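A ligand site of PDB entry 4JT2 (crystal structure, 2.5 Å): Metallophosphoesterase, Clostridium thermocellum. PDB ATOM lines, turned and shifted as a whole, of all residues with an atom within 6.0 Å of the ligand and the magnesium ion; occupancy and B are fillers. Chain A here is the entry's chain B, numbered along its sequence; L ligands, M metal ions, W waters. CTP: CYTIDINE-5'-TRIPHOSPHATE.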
ATOM      1  N   GLY A  16      19.206  22.128 -11.653  1.00  0.00           N
ATOM      2  CA  GLY A  16      20.245  22.335 -10.661  1.00  0.00           C
ATOM      3  C   GLY A  16      19.934  23.444  -9.677  1.00  0.00           C
ATOM      4  O   GLY A  16      19.168  24.371  -9.967  1.00  0.00           O
ATOM      5  N   SER A  17      20.528  23.327  -8.497  1.00  0.00           N
ATOM      6  CA  SER A  17      20.414  24.322  -7.456  1.00  0.00           C
ATOM      7  C   SER A  17      20.904  25.686  -7.923  1.00  0.00           C
ATOM      8  O   SER A  17      21.591  25.810  -8.927  1.00  0.00           O
ATOM      9  CB  SER A  17      21.258  23.899  -6.262  1.00  0.00           C
ATOM     10  OG  SER A  17      21.238  24.882  -5.253  1.00  0.00           O
ATOM     11  N   SER A  18      20.527  26.720  -7.203  1.00  0.00           N
ATOM     12  CA  SER A  18      21.175  28.010  -7.399  1.00  0.00           C
ATOM     13  C   SER A  18      22.658  27.812  -7.096  1.00  0.00           C
ATOM     14  O   SER A  18      23.034  27.105  -6.150  1.00  0.00           O
ATOM     15  CB  SER A  18      20.577  29.043  -6.466  1.00  0.00           C
ATOM     16  OG  SER A  18      21.180  30.314  -6.689  1.00  0.00           O
ATOM     17  N   GLY A  19      23.518  28.417  -7.906  1.00  0.00           N
ATOM     18  CA  GLY A  19      24.956  28.289  -7.724  1.00  0.00           C
ATOM     19  C   GLY A  19      25.555  27.072  -8.439  1.00  0.00           C
ATOM     20  O   GLY A  19      26.777  26.933  -8.490  1.00  0.00           O
ATOM     21  N   SER A  20      24.727  26.210  -8.998  1.00  0.00           N
ATOM     22  CA  SER A  20      25.244  25.004  -9.643  1.00  0.00           C
ATOM     23  C   SER A  20      25.878  25.323 -11.005  1.00  0.00           C
ATOM     24  O   SER A  20      26.604  24.502 -11.565  1.00  0.00           O
ATOM     25  CB  SER A  20      24.164  23.916  -9.760  1.00  0.00           C
ATOM     26  OG  SER A  20      23.147  24.302 -10.663  1.00  0.00           O
ATOM     27  N   GLY A  21      25.612  26.521 -11.524  1.00  0.00           N
ATOM     28  CA  GLY A  21      26.294  26.985 -12.731  1.00  0.00           C
ATOM     29  C   GLY A  21      25.531  26.852 -14.037  1.00  0.00           C
ATOM     30  O   GLY A  21      26.146  26.814 -15.115  1.00  0.00           O
ATOM     31  N   LYS A  22      24.200  26.824 -13.963  1.00  0.00           N
ATOM     32  CA  LYS A  22      23.348  26.664 -15.145  1.00  0.00           C
ATOM     33  C   LYS A  22      23.535  27.765 -16.201  1.00  0.00           C
ATOM     34  O   LYS A  22      23.765  27.470 -17.374  1.00  0.00           O
ATOM     35  CB  LYS A  22      21.881  26.585 -14.729  1.00  0.00           C
ATOM     36  CG  LYS A  22      21.579  25.450 -13.751  1.00  0.00           C
ATOM     37  CD  LYS A  22      20.120  25.426 -13.358  1.00  0.00           C
ATOM     38  CE  LYS A  22      19.688  26.703 -12.614  1.00  0.00           C
ATOM     39  NZ  LYS A  22      20.338  26.853 -11.290  1.00  0.00           N
ATOM     40  N   SER A  23      23.440  29.027 -15.795  1.00  0.00           N
ATOM     41  CA  SER A  23      23.538  30.137 -16.736  1.00  0.00           C
ATOM     42  C   SER A  23      24.919  30.215 -17.376  1.00  0.00           C
ATOM     43  O   SER A  23      25.062  30.513 -18.571  1.00  0.00           O
ATOM     44  CB  SER A  23      23.179  31.465 -16.048  1.00  0.00           C
ATOM     45  OG  SER A  23      21.889  31.416 -15.481  1.00  0.00           O
ATOM     46  N   THR A  24      25.949  29.950 -16.581  1.00  0.00           N
ATOM     47  CA  THR A  24      27.311  29.897 -17.080  1.00  0.00           C
ATOM     48  C   THR A  24      27.398  28.845 -18.198  1.00  0.00           C
ATOM     49  O   THR A  24      27.966  29.091 -19.264  1.00  0.00           O
ATOM     50  CB  THR A  24      28.304  29.510 -15.958  1.00  0.00           C
ATOM     51  OG1 THR A  24      28.248  30.463 -14.894  1.00  0.00           O
ATOM     52  CG2 THR A  24      29.715  29.456 -16.494  1.00  0.00           C
ATOM     53  N   PHE A  25      26.822  27.681 -17.919  1.00  0.00           N
ATOM     54  CA  PHE A  25      26.768  26.575 -18.863  1.00  0.00           C
ATOM     55  C   PHE A  25      26.010  26.970 -20.139  1.00  0.00           C
ATOM     56  O   PHE A  25      26.524  26.817 -21.259  1.00  0.00           O
ATOM     57  CB  PHE A  25      26.100  25.392 -18.162  1.00  0.00           C
ATOM     58  CG  PHE A  25      26.079  24.120 -18.941  1.00  0.00           C
ATOM     59  CD1 PHE A  25      24.989  23.772 -19.717  1.00  0.00           C
ATOM     60  CD2 PHE A  25      27.126  23.223 -18.851  1.00  0.00           C
ATOM     61  CE1 PHE A  25      24.962  22.574 -20.418  1.00  0.00           C
ATOM     62  CE2 PHE A  25      27.107  22.029 -19.556  1.00  0.00           C
ATOM     63  CZ  PHE A  25      26.016  21.704 -20.331  1.00  0.00           C
ATOM     64  N   ASP A  39      14.934  34.387 -14.461  1.00  0.00           N
ATOM     65  CA  ASP A  39      15.256  35.745 -14.047  1.00  0.00           C
ATOM     66  C   ASP A  39      14.947  36.777 -15.115  1.00  0.00           C
ATOM     67  O   ASP A  39      14.498  37.868 -14.803  1.00  0.00           O
ATOM     68  CB  ASP A  39      16.713  35.878 -13.623  1.00  0.00           C
ATOM     69  CG  ASP A  39      17.039  34.995 -12.452  1.00  0.00           C
ATOM     70  OD1 ASP A  39      16.167  34.852 -11.565  1.00  0.00           O
ATOM     71  OD2 ASP A  39      18.150  34.435 -12.431  1.00  0.00           O
ATOM     72  N   ASP A  79      16.679  27.937 -18.738  1.00  0.00           N
ATOM     73  CA  ASP A  79      17.608  28.202 -17.644  1.00  0.00           C
ATOM     74  C   ASP A  79      16.838  28.556 -16.380  1.00  0.00           C
ATOM     75  O   ASP A  79      16.592  29.722 -16.125  1.00  0.00           O
ATOM     76  CB  ASP A  79      18.558  29.325 -18.041  1.00  0.00           C
ATOM     77  CG  ASP A  79      19.562  29.644 -16.952  1.00  0.00           C
ATOM     78  OD1 ASP A  79      19.686  28.858 -15.995  1.00  0.00           O
ATOM     79  OD2 ASP A  79      20.231  30.685 -17.064  1.00  0.00           O
ATOM     80  N   ALA A  80      16.452  27.546 -15.613  1.00  0.00           N
ATOM     81  CA  ALA A  80      15.810  27.758 -14.333  1.00  0.00           C
ATOM     82  C   ALA A  80      16.232  26.620 -13.411  1.00  0.00           C
ATOM     83  O   ALA A  80      16.853  25.664 -13.875  1.00  0.00           O
ATOM     84  CB  ALA A  80      14.301  27.775 -14.493  1.00  0.00           C
ATOM     85  N   THR A  81      15.907  26.714 -12.125  1.00  0.00           N
ATOM     86  CA  THR A  81      16.324  25.674 -11.188  1.00  0.00           C
ATOM     87  C   THR A  81      15.744  24.317 -11.609  1.00  0.00           C
ATOM     88  O   THR A  81      16.476  23.349 -11.720  1.00  0.00           O
ATOM     89  CB  THR A  81      15.916  25.990  -9.743  1.00  0.00           C
ATOM     90  OG1 THR A  81      14.490  25.983  -9.625  1.00  0.00           O
ATOM     91  CG2 THR A  81      16.452  27.350  -9.339  1.00  0.00           C
ATOM     92  N   ARG A 117      30.143  28.912  -4.443  1.00  0.00           N
ATOM     93  CA  ARG A 117      30.034  29.783  -5.604  1.00  0.00           C
ATOM     94  C   ARG A 117      29.084  30.931  -5.309  1.00  0.00           C
ATOM     95  O   ARG A 117      29.317  32.081  -5.693  1.00  0.00           O
ATOM     96  CB  ARG A 117      29.547  29.020  -6.826  1.00  0.00           C
ATOM     97  CG  ARG A 117      30.506  27.957  -7.344  1.00  0.00           C
ATOM     98  CD  ARG A 117      29.873  27.143  -8.476  1.00  0.00           C
ATOM     99  NE  ARG A 117      30.834  26.302  -9.170  1.00  0.00           N
ATOM    100  CZ  ARG A 117      30.518  25.412 -10.105  1.00  0.00           C
ATOM    101  NH1 ARG A 117      29.250  25.242 -10.468  1.00  0.00           N
ATOM    102  NH2 ARG A 117      31.470  24.677 -10.667  1.00  0.00           N
ATOM    103  N   ASN A 118      27.989  30.605  -4.624  1.00  0.00           N
ATOM    104  CA  ASN A 118      27.004  31.589  -4.183  1.00  0.00           C
ATOM    105  C   ASN A 118      27.624  32.742  -3.389  1.00  0.00           C
ATOM    106  O   ASN A 118      27.324  33.901  -3.644  1.00  0.00           O
ATOM    107  CB  ASN A 118      25.934  30.909  -3.334  1.00  0.00           C
ATOM    108  CG  ASN A 118      24.835  31.847  -2.918  1.00  0.00           C
ATOM    109  OD1 ASN A 118      24.251  32.543  -3.741  1.00  0.00           O
ATOM    110  ND2 ASN A 118      24.557  31.884  -1.628  1.00  0.00           N
ATOM    111  N   ASN A 120      30.417  33.948  -3.569  1.00  0.00           N
ATOM    112  CA  ASN A 120      31.345  34.718  -4.389  1.00  0.00           C
ATOM    113  C   ASN A 120      30.715  35.369  -5.619  1.00  0.00           C
ATOM    114  O   ASN A 120      31.398  36.053  -6.378  1.00  0.00           O
ATOM    115  CB  ASN A 120      32.535  33.838  -4.792  1.00  0.00           C
ATOM    116  CG  ASN A 120      33.419  33.462  -3.611  1.00  0.00           C
ATOM    117  OD1 ASN A 120      33.784  34.296  -2.779  1.00  0.00           O
ATOM    118  ND2 ASN A 120      33.771  32.181  -3.535  1.00  0.00           N
ATOM    119  N   ARG A 121      29.418  35.151  -5.825  1.00  0.00           N
ATOM    120  CA  ARG A 121      28.692  35.770  -6.928  1.00  0.00           C
ATOM    121  C   ARG A 121      28.701  37.285  -6.806  1.00  0.00           C
ATOM    122  O   ARG A 121      28.596  37.813  -5.713  1.00  0.00           O
ATOM    123  CB  ARG A 121      27.243  35.282  -6.950  1.00  0.00           C
ATOM    124  CG  ARG A 121      27.102  33.812  -7.132  1.00  0.00           C
ATOM    125  CD  ARG A 121      25.643  33.450  -7.285  1.00  0.00           C
ATOM    126  NE  ARG A 121      25.048  34.065  -8.475  1.00  0.00           N
ATOM    127  CZ  ARG A 121      23.950  33.594  -9.060  1.00  0.00           C
ATOM    128  NH1 ARG A 121      23.347  32.511  -8.569  1.00  0.00           N
ATOM    129  NH2 ARG A 121      23.452  34.191 -10.136  1.00  0.00           N
ATOM    130  N   THR A 122      28.788  37.967  -7.942  1.00  0.00           N
ATOM    131  CA  THR A 122      28.741  39.427  -7.981  1.00  0.00           C
ATOM    132  C   THR A 122      27.403  39.945  -8.507  1.00  0.00           C
ATOM    133  O   THR A 122      27.151  41.149  -8.460  1.00  0.00           O
ATOM    134  CB  THR A 122      29.863  40.003  -8.861  1.00  0.00           C
ATOM    135  OG1 THR A 122      29.799  39.416 -10.172  1.00  0.00           O
ATOM    136  CG2 THR A 122      31.216  39.707  -8.251  1.00  0.00           C
ATOM    137  N   ASP A 123      26.569  39.058  -9.022  1.00  0.00           N
ATOM    138  CA  ASP A 123      25.296  39.491  -9.582  1.00  0.00           C
ATOM    139  C   ASP A 123      24.185  39.501  -8.547  1.00  0.00           C
ATOM    140  O   ASP A 123      23.562  40.537  -8.313  1.00  0.00           O
ATOM    141  CB  ASP A 123      24.911  38.670 -10.820  1.00  0.00           C
ATOM    142  CG  ASP A 123      25.119  37.178 -10.646  1.00  0.00           C
ATOM    143  OD1 ASP A 123      25.891  36.775  -9.745  1.00  0.00           O
ATOM    144  OD2 ASP A 123      24.524  36.415 -11.420  1.00  0.00           O
ATOM    145  N   ARG A 124      23.941  38.363  -7.916  1.00  0.00           N
ATOM    146  CA  ARG A 124      22.944  38.257  -6.858  1.00  0.00           C
ATOM    147  C   ARG A 124      23.250  37.010  -6.047  1.00  0.00           C
ATOM    148  O   ARG A 124      23.862  36.082  -6.560  1.00  0.00           O
ATOM    149  CB  ARG A 124      21.535  38.151  -7.457  1.00  0.00           C
ATOM    150  CG  ARG A 124      21.407  37.011  -8.430  1.00  0.00           C
ATOM    151  CD  ARG A 124      20.053  36.965  -9.120  1.00  0.00           C
ATOM    152  NE  ARG A 124      20.099  36.019 -10.243  1.00  0.00           N
ATOM    153  CZ  ARG A 124      19.914  34.706 -10.121  1.00  0.00           C
ATOM    154  NH1 ARG A 124      19.660  34.166  -8.936  1.00  0.00           N
ATOM    155  NH2 ARG A 124      19.991  33.938 -11.188  1.00  0.00           N
ATOM    156  N   VAL A 126      21.651  34.122  -2.905  1.00  0.00           N
ATOM    157  CA  VAL A 126      20.510  33.600  -2.166  1.00  0.00           C
ATOM    158  C   VAL A 126      20.926  33.170  -0.774  1.00  0.00           C
ATOM    159  O   VAL A 126      22.118  33.031  -0.507  1.00  0.00           O
ATOM    160  CB  VAL A 126      19.840  32.406  -2.891  1.00  0.00           C
ATOM    161  CG1 VAL A 126      19.475  32.776  -4.313  1.00  0.00           C
ATOM    162  CG2 VAL A 126      20.744  31.168  -2.865  1.00  0.00           C
ATOM    163  N   VAL A 162      31.061  18.516 -15.936  1.00  0.00           N
ATOM    164  CA  VAL A 162      30.368  19.684 -16.479  1.00  0.00           C
ATOM    165  C   VAL A 162      31.266  20.437 -17.458  1.00  0.00           C
ATOM    166  O   VAL A 162      30.824  20.867 -18.524  1.00  0.00           O
ATOM    167  CB  VAL A 162      29.958  20.645 -15.368  1.00  0.00           C
ATOM    168  CG1 VAL A 162      29.436  21.949 -15.956  1.00  0.00           C
ATOM    169  CG2 VAL A 162      28.934  19.987 -14.450  1.00  0.00           C
ATOM    170  N   GLU A 163      32.525  20.574 -17.071  1.00  0.00           N
ATOM    171  CA  GLU A 163      33.515  21.271 -17.872  1.00  0.00           C
ATOM    172  C   GLU A 163      33.750  20.589 -19.223  1.00  0.00           C
ATOM    173  O   GLU A 163      33.906  21.253 -20.257  1.00  0.00           O
ATOM    174  CB  GLU A 163      34.827  21.334 -17.093  1.00  0.00           C
ATOM    175  CG  GLU A 163      35.265  22.726 -16.707  1.00  0.00           C
ATOM    176  CD  GLU A 163      35.987  23.440 -17.849  1.00  0.00           C
ATOM    177  OE1 GLU A 163      36.287  24.646 -17.705  1.00  0.00           O
ATOM    178  OE2 GLU A 163      36.256  22.779 -18.874  1.00  0.00           O
HETATM  179  N1  CTP L   1      30.894  29.452 -11.379  1.00  0.00           N
HETATM  180  C2  CTP L   1      32.252  29.091 -11.460  1.00  0.00           C
HETATM  181  N3  CTP L   1      32.634  28.120 -12.307  1.00  0.00           N
HETATM  182  C4  CTP L   1      31.723  27.490 -13.097  1.00  0.00           C
HETATM  183  C5  CTP L   1      30.378  27.847 -13.021  1.00  0.00           C
HETATM  184  C6  CTP L   1      29.983  28.852 -12.148  1.00  0.00           C
HETATM  185  O2  CTP L   1      33.098  29.675 -10.733  1.00  0.00           O
HETATM  186  N4  CTP L   1      32.118  26.515 -13.949  1.00  0.00           N
HETATM  187  C1' CTP L   1      30.526  30.520 -10.461  1.00  0.00           C
HETATM  188  C2' CTP L   1      30.594  31.816 -11.261  1.00  0.00           C
HETATM  189  O2' CTP L   1      31.784  32.531 -10.945  1.00  0.00           O
HETATM  190  C3' CTP L   1      29.371  32.596 -10.849  1.00  0.00           C
HETATM  191  C4' CTP L   1      28.591  31.685  -9.913  1.00  0.00           C
HETATM  192  O4' CTP L   1      29.185  30.391  -9.973  1.00  0.00           O
HETATM  193  O3' CTP L   1      29.757  33.795 -10.164  1.00  0.00           O
HETATM  194  C5' CTP L   1      27.142  31.594 -10.350  1.00  0.00           C
HETATM  195  O5' CTP L   1      26.965  30.596 -11.356  1.00  0.00           O
HETATM  196  PA  CTP L   1      25.635  30.654 -12.263  1.00  0.00           P
HETATM  197  O1A CTP L   1      25.936  30.092 -13.635  1.00  0.00           O
HETATM  198  O2A CTP L   1      25.021  32.022 -12.164  1.00  0.00           O
HETATM  199  O3A CTP L   1      24.732  29.606 -11.437  1.00  0.00           O
HETATM  200  PB  CTP L   1      23.179  29.403 -11.766  1.00  0.00           P
HETATM  201  O1B CTP L   1      22.945  27.915 -11.822  1.00  0.00           O
HETATM  202  O2B CTP L   1      22.841  30.250 -12.966  1.00  0.00           O
HETATM  203  O3B CTP L   1      22.470  29.995 -10.434  1.00  0.00           O
HETATM  204  PG  CTP L   1      20.971  30.632 -10.384  1.00  0.00           P
HETATM  205  O1G CTP L   1      20.012  29.461 -10.397  1.00  0.00           O
HETATM  206  O2G CTP L   1      20.984  31.378  -9.084  1.00  0.00           O
HETATM  207  O3G CTP L   1      20.868  31.519 -11.610  1.00  0.00           O
HETATM  208 MG    MG M   1      21.586  31.644 -13.439  1.00  0.00          MG
HETATM  209  O   HOH W   1      22.938  33.191 -12.982  1.00  0.00           O
HETATM  210  O   HOH W   2      19.966  30.303 -13.853  1.00  0.00           O
HETATM  211  O   HOH W   3      31.148  32.560  -7.958  1.00  0.00           O
HETATM  212  O   HOH W   4      30.111  36.675 -10.503  1.00  0.00           O
HETATM  213  O   HOH W   5      19.887  32.895 -14.155  1.00  0.00           O
HETATM  214  O   HOH W   6      26.447  34.436 -12.540  1.00  0.00           O
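The backbone NH of Gly 19 sits at hydrogen-bond distance from an oxygen (O3B) of the ligand (3.2 Å).
An oxygen (O1A) of the ligand is in hydrogen-bond range of the backbone NH of Thr 24, 2.9 Å away.
O1A of the ligand lies within hydrogen-bond range of OG1 of Thr 24 (2.7 Å).
N of Lys 22 lies within hydrogen-bond range of O1B of the ligand (2.7 Å).
The backbone NH of Gly 21 is in hydrogen-bond range of an oxygen (O1B) of the ligand.
An oxygen (O2G) of the ligand lies within salt-bridge range of the guanidinium group (NH1) of Arg 124, at 3.1 Å.
The backbone NH (N) of Ser 23 lies within hydrogen-bond range of an oxygen (O1A) of the ligand (3.5 Å).
The guanidinium group (NH1) of Arg 121 is in salt-bridge range of an oxygen (O2G) of the ligand, at 2.7 Å.
The side-chain amino group (NZ) of Lys 22 lies within salt-bridge range of an oxygen (O1G) of the ligand (2.8 Å).
An oxygen (O2G) of the ligand sits at hydrogen-bond distance from the side-chain hydroxyl (OG) of Ser 18 (2.6 Å).
The guanidinium group (NE) of Arg 124 lies within salt-bridge range of the side-chain carboxylate (OD2) of Asp 39 (3.3 Å).
OG of Ser 20 lies within hydrogen-bond range of O of Ser 17, 2.8 Å away.
The backbone carbonyl oxygen (O) of Ser 20 lies within hydrogen-bond range of the guanidinium group (NH1) of Arg 117 (3.0 Å).
NZ of Lys 22 sits at hydrogen-bond distance from O of Ser 17, 2.9 Å away.
The side-chain carboxylate (OD2) of Asp 123 is in salt-bridge range of the guanidinium group (NH2) of Arg 121, 2.8 Å away.
The guanidinium group (NE) of Arg 121 sits at hydrogen-bond distance from the backbone carbonyl oxygen (O) of Arg 124 (3.0 Å).
The side-chain amino group (NZ) of Lys 22 is in hydrogen-bond range of the backbone carbonyl oxygen (O) of Gly 16 (3.0 Å).
OG of Ser 23 lies close to OD2 of Asp 79, 2.4 Å away.
Ser 17 touches the ligand (O to O1B, 3.8 Å).
Ser 20 touches the ligand (N to O1B, 3.7 Å).
Arg 117 touches the ligand (CB to O4', 3.5 Å).
Of the 24 residues printed, 11 come within 4 Å of the ligand.
Residues that only touch the magnesium ion: Arg 124 (3.6 Å) and Asp 79 (3.99 Å).
The magnesium ion is bound by an oxygen (O2B) of the ligand (1.9 Å), an oxygen (O3G) of the ligand (2.0 Å), the side-chain hydroxyl of Ser 23 (2.1 Å), water W1 (2.1 Å), water W2 (2.1 Å) and water W5 (2.2 Å).
The magnesium ion has six donor atoms within binding distance.
Water W5 bridges the side-chain carboxylate (OD2) of Asp 39 (2.9 Å) and the guanidinium group (NH2) of Arg 124 (3.1 Å).
Water W1 bridges an oxygen (O2A) of the ligand (2.5 Å) and the guanidinium group of Arg 121 (3.1 Å).
Water W6 bridges an oxygen (O2A) of the ligand (2.8 Å) and the side-chain carboxylate of Asp 123 (3.0 Å).
Water W3 lies within hydrogen-bond range of O3' of the ligand (2.9 Å) and O of Arg 117 (3.0 Å).
Water W4 bridges OG1 of Thr 122 (2.8 Å) and O3' of the ligand (2.9 Å).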
